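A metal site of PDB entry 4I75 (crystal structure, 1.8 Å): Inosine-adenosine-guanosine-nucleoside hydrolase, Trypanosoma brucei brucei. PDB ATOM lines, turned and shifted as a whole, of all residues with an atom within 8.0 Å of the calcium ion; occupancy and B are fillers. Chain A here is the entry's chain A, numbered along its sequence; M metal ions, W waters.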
ATOM      1  N   ASP A  11      33.925  27.444  23.240  1.00  0.00           N
ATOM      2  CA  ASP A  11      34.560  26.179  23.605  1.00  0.00           C
ATOM      3  C   ASP A  11      33.425  25.131  23.487  1.00  0.00           C
ATOM      4  O   ASP A  11      32.590  24.984  24.379  1.00  0.00           O
ATOM      5  CB  ASP A  11      35.160  26.358  25.003  1.00  0.00           C
ATOM      6  CG  ASP A  11      35.688  25.097  25.666  1.00  0.00           C
ATOM      7  OD1 ASP A  11      35.644  23.955  25.075  1.00  0.00           O
ATOM      8  OD2 ASP A  11      36.146  25.270  26.817  1.00  0.00           O
ATOM      9  N   HIS A  12      33.399  24.401  22.365  1.00  0.00           N
ATOM     10  CA  HIS A  12      32.201  23.590  21.978  1.00  0.00           C
ATOM     11  C   HIS A  12      32.577  22.136  21.657  1.00  0.00           C
ATOM     12  O   HIS A  12      33.731  21.809  21.525  1.00  0.00           O
ATOM     13  CB  HIS A  12      31.423  24.229  20.836  1.00  0.00           C
ATOM     14  CG  HIS A  12      32.091  24.148  19.507  1.00  0.00           C
ATOM     15  ND1 HIS A  12      32.017  23.027  18.729  1.00  0.00           N
ATOM     16  CD2 HIS A  12      32.809  25.064  18.793  1.00  0.00           C
ATOM     17  CE1 HIS A  12      32.676  23.221  17.594  1.00  0.00           C
ATOM     18  NE2 HIS A  12      33.176  24.447  17.622  1.00  0.00           N
ATOM     19  N   ASP A  13      31.581  21.277  21.544  1.00  0.00           N
ATOM     20  CA  ASP A  13      31.800  19.910  21.131  1.00  0.00           C
ATOM     21  C   ASP A  13      30.957  19.445  19.976  1.00  0.00           C
ATOM     22  O   ASP A  13      30.585  18.252  19.865  1.00  0.00           O
ATOM     23  CB  ASP A  13      31.651  18.943  22.347  1.00  0.00           C
ATOM     24  CG  ASP A  13      30.251  18.865  22.877  1.00  0.00           C
ATOM     25  OD1 ASP A  13      29.423  19.725  22.550  1.00  0.00           O
ATOM     26  OD2 ASP A  13      29.952  17.885  23.658  1.00  0.00           O
ATOM     27  N   GLY A  14      30.679  20.378  19.059  1.00  0.00           N
ATOM     28  CA  GLY A  14      30.403  19.976  17.682  1.00  0.00           C
ATOM     29  C   GLY A  14      29.095  19.330  17.290  1.00  0.00           C
ATOM     30  O   GLY A  14      29.055  18.612  16.283  1.00  0.00           O
ATOM     31  N   ASN A  15      28.013  19.570  18.035  1.00  0.00           N
ATOM     32  CA  ASN A  15      26.700  19.077  17.613  1.00  0.00           C
ATOM     33  C   ASN A  15      25.807  20.262  17.165  1.00  0.00           C
ATOM     34  O   ASN A  15      26.270  21.418  17.116  1.00  0.00           O
ATOM     35  CB  ASN A  15      26.002  18.169  18.668  1.00  0.00           C
ATOM     36  CG  ASN A  15      25.271  16.976  18.016  1.00  0.00           C
ATOM     37  OD1 ASN A  15      24.335  17.173  17.227  1.00  0.00           O
ATOM     38  ND2 ASN A  15      25.708  15.746  18.335  1.00  0.00           N
ATOM     39  N   LYS A  16      24.552  19.946  16.846  1.00  0.00           N
ATOM     40  CA  LYS A  16      23.662  20.903  16.231  1.00  0.00           C
ATOM     41  C   LYS A  16      23.408  22.106  17.185  1.00  0.00           C
ATOM     42  O   LYS A  16      23.400  23.274  16.768  1.00  0.00           O
ATOM     43  CB  LYS A  16      22.365  20.216  15.770  1.00  0.00           C
ATOM     44  CG  LYS A  16      22.558  19.218  14.636  1.00  0.00           C
ATOM     45  CD  LYS A  16      21.376  18.357  14.316  1.00  0.00           C
ATOM     46  CE  LYS A  16      21.019  17.353  15.425  1.00  0.00           C
ATOM     47  NZ  LYS A  16      22.060  16.327  15.660  1.00  0.00           N
ATOM     48  N   ASP A  17      23.192  21.806  18.462  1.00  0.00           N
ATOM     49  CA  ASP A  17      23.071  22.855  19.467  1.00  0.00           C
ATOM     50  C   ASP A  17      24.329  23.757  19.565  1.00  0.00           C
ATOM     51  O   ASP A  17      24.235  24.995  19.666  1.00  0.00           O
ATOM     52  CB  ASP A  17      22.601  22.276  20.815  1.00  0.00           C
ATOM     53  CG  ASP A  17      23.467  21.096  21.319  1.00  0.00           C
ATOM     54  OD1 ASP A  17      24.356  20.608  20.619  1.00  0.00           O
ATOM     55  OD2 ASP A  17      23.215  20.667  22.460  1.00  0.00           O
ATOM     56  N   ASP A  18      25.519  23.164  19.517  1.00  0.00           N
ATOM     57  CA  ASP A  18      26.764  23.948  19.525  1.00  0.00           C
ATOM     58  C   ASP A  18      26.851  24.923  18.318  1.00  0.00           C
ATOM     59  O   ASP A  18      27.304  26.084  18.440  1.00  0.00           O
ATOM     60  CB  ASP A  18      27.980  23.016  19.512  1.00  0.00           C
ATOM     61  CG  ASP A  18      28.006  22.069  20.679  1.00  0.00           C
ATOM     62  OD1 ASP A  18      28.608  22.400  21.731  1.00  0.00           O
ATOM     63  OD2 ASP A  18      27.457  20.984  20.571  1.00  0.00           O
ATOM     64  N   PHE A  19      26.422  24.462  17.152  1.00  0.00           N
ATOM     65  CA  PHE A  19      26.507  25.293  15.953  1.00  0.00           C
ATOM     66  C   PHE A  19      25.444  26.360  15.887  1.00  0.00           C
ATOM     67  O   PHE A  19      25.685  27.411  15.295  1.00  0.00           O
ATOM     68  CB  PHE A  19      26.615  24.454  14.695  1.00  0.00           C
ATOM     69  CG  PHE A  19      27.897  23.623  14.668  1.00  0.00           C
ATOM     70  CD1 PHE A  19      29.164  24.250  14.736  1.00  0.00           C
ATOM     71  CD2 PHE A  19      27.857  22.253  14.570  1.00  0.00           C
ATOM     72  CE1 PHE A  19      30.338  23.539  14.713  1.00  0.00           C
ATOM     73  CE2 PHE A  19      29.033  21.513  14.543  1.00  0.00           C
ATOM     74  CZ  PHE A  19      30.277  22.174  14.621  1.00  0.00           C
ATOM     75  N   ALA A  21      24.513  27.863  18.637  1.00  0.00           N
ATOM     76  CA  ALA A  21      25.253  28.822  19.496  1.00  0.00           C
ATOM     77  C   ALA A  21      26.317  29.613  18.731  1.00  0.00           C
ATOM     78  O   ALA A  21      26.395  30.873  18.818  1.00  0.00           O
ATOM     79  CB  ALA A  21      25.909  28.100  20.770  1.00  0.00           C
ATOM     80  N   THR A  40      35.971  19.963  20.985  1.00  0.00           N
ATOM     81  CA  THR A  40      36.307  18.777  21.788  1.00  0.00           C
ATOM     82  C   THR A  40      35.542  17.519  21.294  1.00  0.00           C
ATOM     83  O   THR A  40      34.385  17.616  20.877  1.00  0.00           O
ATOM     84  CB  THR A  40      35.925  19.017  23.271  1.00  0.00           C
ATOM     85  OG1 THR A  40      36.700  20.119  23.759  1.00  0.00           O
ATOM     86  CG2 THR A  40      36.251  17.788  24.181  1.00  0.00           C
ATOM     87  N   ALA A  42      33.713  15.193  22.110  1.00  0.00           N
ATOM     88  CA  ALA A  42      32.716  14.724  23.083  1.00  0.00           C
ATOM     89  C   ALA A  42      31.391  14.339  22.374  1.00  0.00           C
ATOM     90  O   ALA A  42      31.248  13.201  22.016  1.00  0.00           O
ATOM     91  CB  ALA A  42      32.530  15.781  24.212  1.00  0.00           C
ATOM     92  N   ASP A  43      30.452  15.304  22.163  1.00  0.00           N
ATOM     93  CA  ASP A  43      29.189  15.085  21.361  1.00  0.00           C
ATOM     94  C   ASP A  43      29.397  15.138  19.841  1.00  0.00           C
ATOM     95  O   ASP A  43      28.488  15.489  19.091  1.00  0.00           O
ATOM     96  CB  ASP A  43      28.150  16.112  21.787  1.00  0.00           C
ATOM     97  CG  ASP A  43      26.705  15.738  21.482  1.00  0.00           C
ATOM     98  OD1 ASP A  43      26.331  14.576  21.296  1.00  0.00           O
ATOM     99  OD2 ASP A  43      25.868  16.674  21.451  1.00  0.00           O
ATOM    100  N   CYS A  44      30.602  14.761  19.399  1.00  0.00           N
ATOM    101  CA  CYS A  44      31.007  14.694  17.978  1.00  0.00           C
ATOM    102  C   CYS A  44      32.239  13.816  17.888  1.00  0.00           C
ATOM    103  O   CYS A  44      32.767  13.334  18.944  1.00  0.00           O
ATOM    104  CB  CYS A  44      31.327  16.098  17.408  1.00  0.00           C
ATOM    105  SG  CYS A  44      32.914  16.805  17.875  1.00  0.00           S
ATOM    106  N   PHE A  82      30.151  10.053  25.214  1.00  0.00           N
ATOM    107  CA  PHE A  82      28.817  10.232  24.730  1.00  0.00           C
ATOM    108  C   PHE A  82      28.376   9.006  23.947  1.00  0.00           C
ATOM    109  O   PHE A  82      29.162   8.293  23.378  1.00  0.00           O
ATOM    110  CB  PHE A  82      28.654  11.467  23.803  1.00  0.00           C
ATOM    111  CG  PHE A  82      28.392  12.773  24.512  1.00  0.00           C
ATOM    112  CD1 PHE A  82      27.145  13.288  24.572  1.00  0.00           C
ATOM    113  CD2 PHE A  82      29.413  13.468  25.086  1.00  0.00           C
ATOM    114  CE1 PHE A  82      26.874  14.506  25.232  1.00  0.00           C
ATOM    115  CE2 PHE A  82      29.161  14.693  25.756  1.00  0.00           C
ATOM    116  CZ  PHE A  82      27.894  15.207  25.814  1.00  0.00           C
ATOM    117  N   VAL A 139      30.994  28.035  27.050  1.00  0.00           N
ATOM    118  CA  VAL A 139      31.303  26.615  27.099  1.00  0.00           C
ATOM    119  C   VAL A 139      30.022  25.783  26.829  1.00  0.00           C
ATOM    120  O   VAL A 139      29.128  25.778  27.641  1.00  0.00           O
ATOM    121  CB  VAL A 139      31.945  26.191  28.434  1.00  0.00           C
ATOM    122  CG1 VAL A 139      32.319  24.701  28.395  1.00  0.00           C
ATOM    123  CG2 VAL A 139      33.187  26.990  28.710  1.00  0.00           C
ATOM    124  N   THR A 140      29.966  25.111  25.683  1.00  0.00           N
ATOM    125  CA  THR A 140      28.819  24.343  25.272  1.00  0.00           C
ATOM    126  C   THR A 140      29.071  22.831  25.166  1.00  0.00           C
ATOM    127  O   THR A 140      28.144  22.067  24.851  1.00  0.00           O
ATOM    128  CB  THR A 140      28.261  24.888  23.934  1.00  0.00           C
ATOM    129  OG1 THR A 140      29.223  24.759  22.867  1.00  0.00           O
ATOM    130  CG2 THR A 140      27.879  26.364  24.135  1.00  0.00           C
ATOM    131  N   GLY A 141      30.297  22.419  25.404  1.00  0.00           N
ATOM    132  CA  GLY A 141      30.638  21.022  25.683  1.00  0.00           C
ATOM    133  C   GLY A 141      31.117  20.885  27.139  1.00  0.00           C
ATOM    134  O   GLY A 141      30.798  21.690  27.982  1.00  0.00           O
ATOM    135  N   PRO A 142      31.901  19.834  27.428  1.00  0.00           N
ATOM    136  CA  PRO A 142      32.400  19.576  28.777  1.00  0.00           C
ATOM    137  C   PRO A 142      33.417  20.610  29.218  1.00  0.00           C
ATOM    138  O   PRO A 142      33.911  21.376  28.429  1.00  0.00           O
ATOM    139  CB  PRO A 142      33.091  18.207  28.646  1.00  0.00           C
ATOM    140  CG  PRO A 142      32.280  17.532  27.481  1.00  0.00           C
ATOM    141  CD  PRO A 142      32.195  18.714  26.519  1.00  0.00           C
ATOM    142  N   MET A 167      26.941  25.554  29.592  1.00  0.00           N
ATOM    143  CA  MET A 167      25.842  24.573  29.480  1.00  0.00           C
ATOM    144  C   MET A 167      26.211  23.347  30.280  1.00  0.00           C
ATOM    145  O   MET A 167      27.153  22.626  29.921  1.00  0.00           O
ATOM    146  CB  MET A 167      25.637  24.136  28.026  1.00  0.00           C
ATOM    147  CG  MET A 167      24.686  22.923  27.798  1.00  0.00           C
ATOM    148  SD  MET A 167      22.933  23.329  28.089  1.00  0.00           S
ATOM    149  CE  MET A 167      22.612  22.344  29.570  1.00  0.00           C
ATOM    150  N   GLU A 187      23.704  15.289  34.340  1.00  0.00           N
ATOM    151  CA  GLU A 187      23.620  15.840  32.998  1.00  0.00           C
ATOM    152  C   GLU A 187      24.916  15.533  32.175  1.00  0.00           C
ATOM    153  O   GLU A 187      26.025  15.481  32.715  1.00  0.00           O
ATOM    154  CB  GLU A 187      23.329  17.358  33.093  1.00  0.00           C
ATOM    155  CG  GLU A 187      23.243  18.139  31.740  1.00  0.00           C
ATOM    156  CD  GLU A 187      24.609  18.454  31.123  1.00  0.00           C
ATOM    157  OE1 GLU A 187      25.631  18.597  31.881  1.00  0.00           O
ATOM    158  OE2 GLU A 187      24.664  18.563  29.852  1.00  0.00           O
ATOM    159  N   ASN A 189      27.163  16.943  29.817  1.00  0.00           N
ATOM    160  CA  ASN A 189      28.389  17.750  29.805  1.00  0.00           C
ATOM    161  C   ASN A 189      29.250  17.575  31.047  1.00  0.00           C
ATOM    162  O   ASN A 189      30.458  17.500  30.935  1.00  0.00           O
ATOM    163  CB  ASN A 189      28.089  19.238  29.564  1.00  0.00           C
ATOM    164  CG  ASN A 189      27.806  19.529  28.072  1.00  0.00           C
ATOM    165  OD1 ASN A 189      27.909  18.630  27.229  1.00  0.00           O
ATOM    166  ND2 ASN A 189      27.459  20.765  27.764  1.00  0.00           N
ATOM    167  N   TRP A 263      19.039  24.102  24.501  1.00  0.00           N
ATOM    168  CA  TRP A 263      20.278  23.682  25.142  1.00  0.00           C
ATOM    169  C   TRP A 263      21.360  24.760  24.935  1.00  0.00           C
ATOM    170  O   TRP A 263      21.189  25.905  25.388  1.00  0.00           O
ATOM    171  CB  TRP A 263      20.737  22.295  24.681  1.00  0.00           C
ATOM    172  CG  TRP A 263      19.989  21.116  25.263  1.00  0.00           C
ATOM    173  CD1 TRP A 263      19.525  20.963  26.526  1.00  0.00           C
ATOM    174  CD2 TRP A 263      19.638  19.922  24.559  1.00  0.00           C
ATOM    175  NE1 TRP A 263      18.904  19.750  26.658  1.00  0.00           N
ATOM    176  CE2 TRP A 263      18.963  19.091  25.469  1.00  0.00           C
ATOM    177  CE3 TRP A 263      19.840  19.474  23.257  1.00  0.00           C
ATOM    178  CZ2 TRP A 263      18.483  17.837  25.109  1.00  0.00           C
ATOM    179  CZ3 TRP A 263      19.368  18.240  22.907  1.00  0.00           C
ATOM    180  CH2 TRP A 263      18.701  17.438  23.822  1.00  0.00           C
ATOM    181  N   ASP A 264      22.453  24.386  24.245  1.00  0.00           N
ATOM    182  CA  ASP A 264      23.623  25.213  24.093  1.00  0.00           C
ATOM    183  C   ASP A 264      23.366  26.617  23.530  1.00  0.00           C
ATOM    184  O   ASP A 264      24.109  27.543  23.868  1.00  0.00           O
ATOM    185  CB  ASP A 264      24.688  24.565  23.176  1.00  0.00           C
ATOM    186  CG  ASP A 264      25.060  23.156  23.621  1.00  0.00           C
ATOM    187  OD1 ASP A 264      24.544  22.709  24.695  1.00  0.00           O
ATOM    188  OD2 ASP A 264      25.853  22.525  22.863  1.00  0.00           O
ATOM    189  N   ALA A 265      22.352  26.730  22.679  1.00  0.00           N
ATOM    190  CA  ALA A 265      22.028  28.007  22.062  1.00  0.00           C
ATOM    191  C   ALA A 265      21.656  29.071  23.142  1.00  0.00           C
ATOM    192  O   ALA A 265      21.832  30.290  22.933  1.00  0.00           O
ATOM    193  CB  ALA A 265      20.911  27.821  21.030  1.00  0.00           C
HETATM  194 CA    CA M   1      27.438  20.700  23.064  1.00  0.00          CA
HETATM  195 NI    NI M   2      24.051  19.004  23.368  1.00  0.00          NI
HETATM  196  O   HOH W   1      25.670  19.092  22.268  1.00  0.00           O
HETATM  197  O   HOH W   2      27.496  18.757  24.544  1.00  0.00           O
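Water W1 lies within hydrogen-bond range of the side-chain carboxylate of Asp 43 (2.6 Å) and the side-chain carboxylate of Asp 17 (2.6 Å).
Water W2 lies within hydrogen-bond range of OD1 of Asn 189 and OD2 of Asp 13.
Residues that only touch the calcium ion: Asp 17 (3.9 Å).
Within 4 Å of the calcium ion: Asp 13, Asp 17, Asp 18, Thr 140 and Asp 264.
The calcium ion is bound by the side-chain carboxylate (OD1) of Asp 13 (2.3 Å), the backbone carbonyl oxygen (O) of Thr 140 (2.4 Å), the side-chain carboxylate (OD2) of Asp 264 (2.4 Å), water W2 (2.4 Å), the side-chain carboxylate (OD1) of Asp 18 (2.5 Å), the side-chain carboxylate (OD2) of Asp 18 (2.5 Å) and water W1 (2.5 Å).
The calcium ion has seven donor atoms within binding distance.
The side-chain carboxylate (OD2) of Asp 13 sits at hydrogen-bond distance from the backbone NH (N) of Asp 43 (3.0 Å).
The backbone carbonyl oxygen of Asp 13 lies close to the side-chain sulfur of Cys 44, at 3.4 Å.
O of Thr 140 lies close to ND2 of Asn 189, 3.3 Å away.
O of Asp 11 sits at hydrogen-bond distance from N of Thr 140 (2.9 Å).
The side-chain carboxylate (OD2) of Asp 18 lies close to the backbone NH (N) of Asn 15 (3.0 Å).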
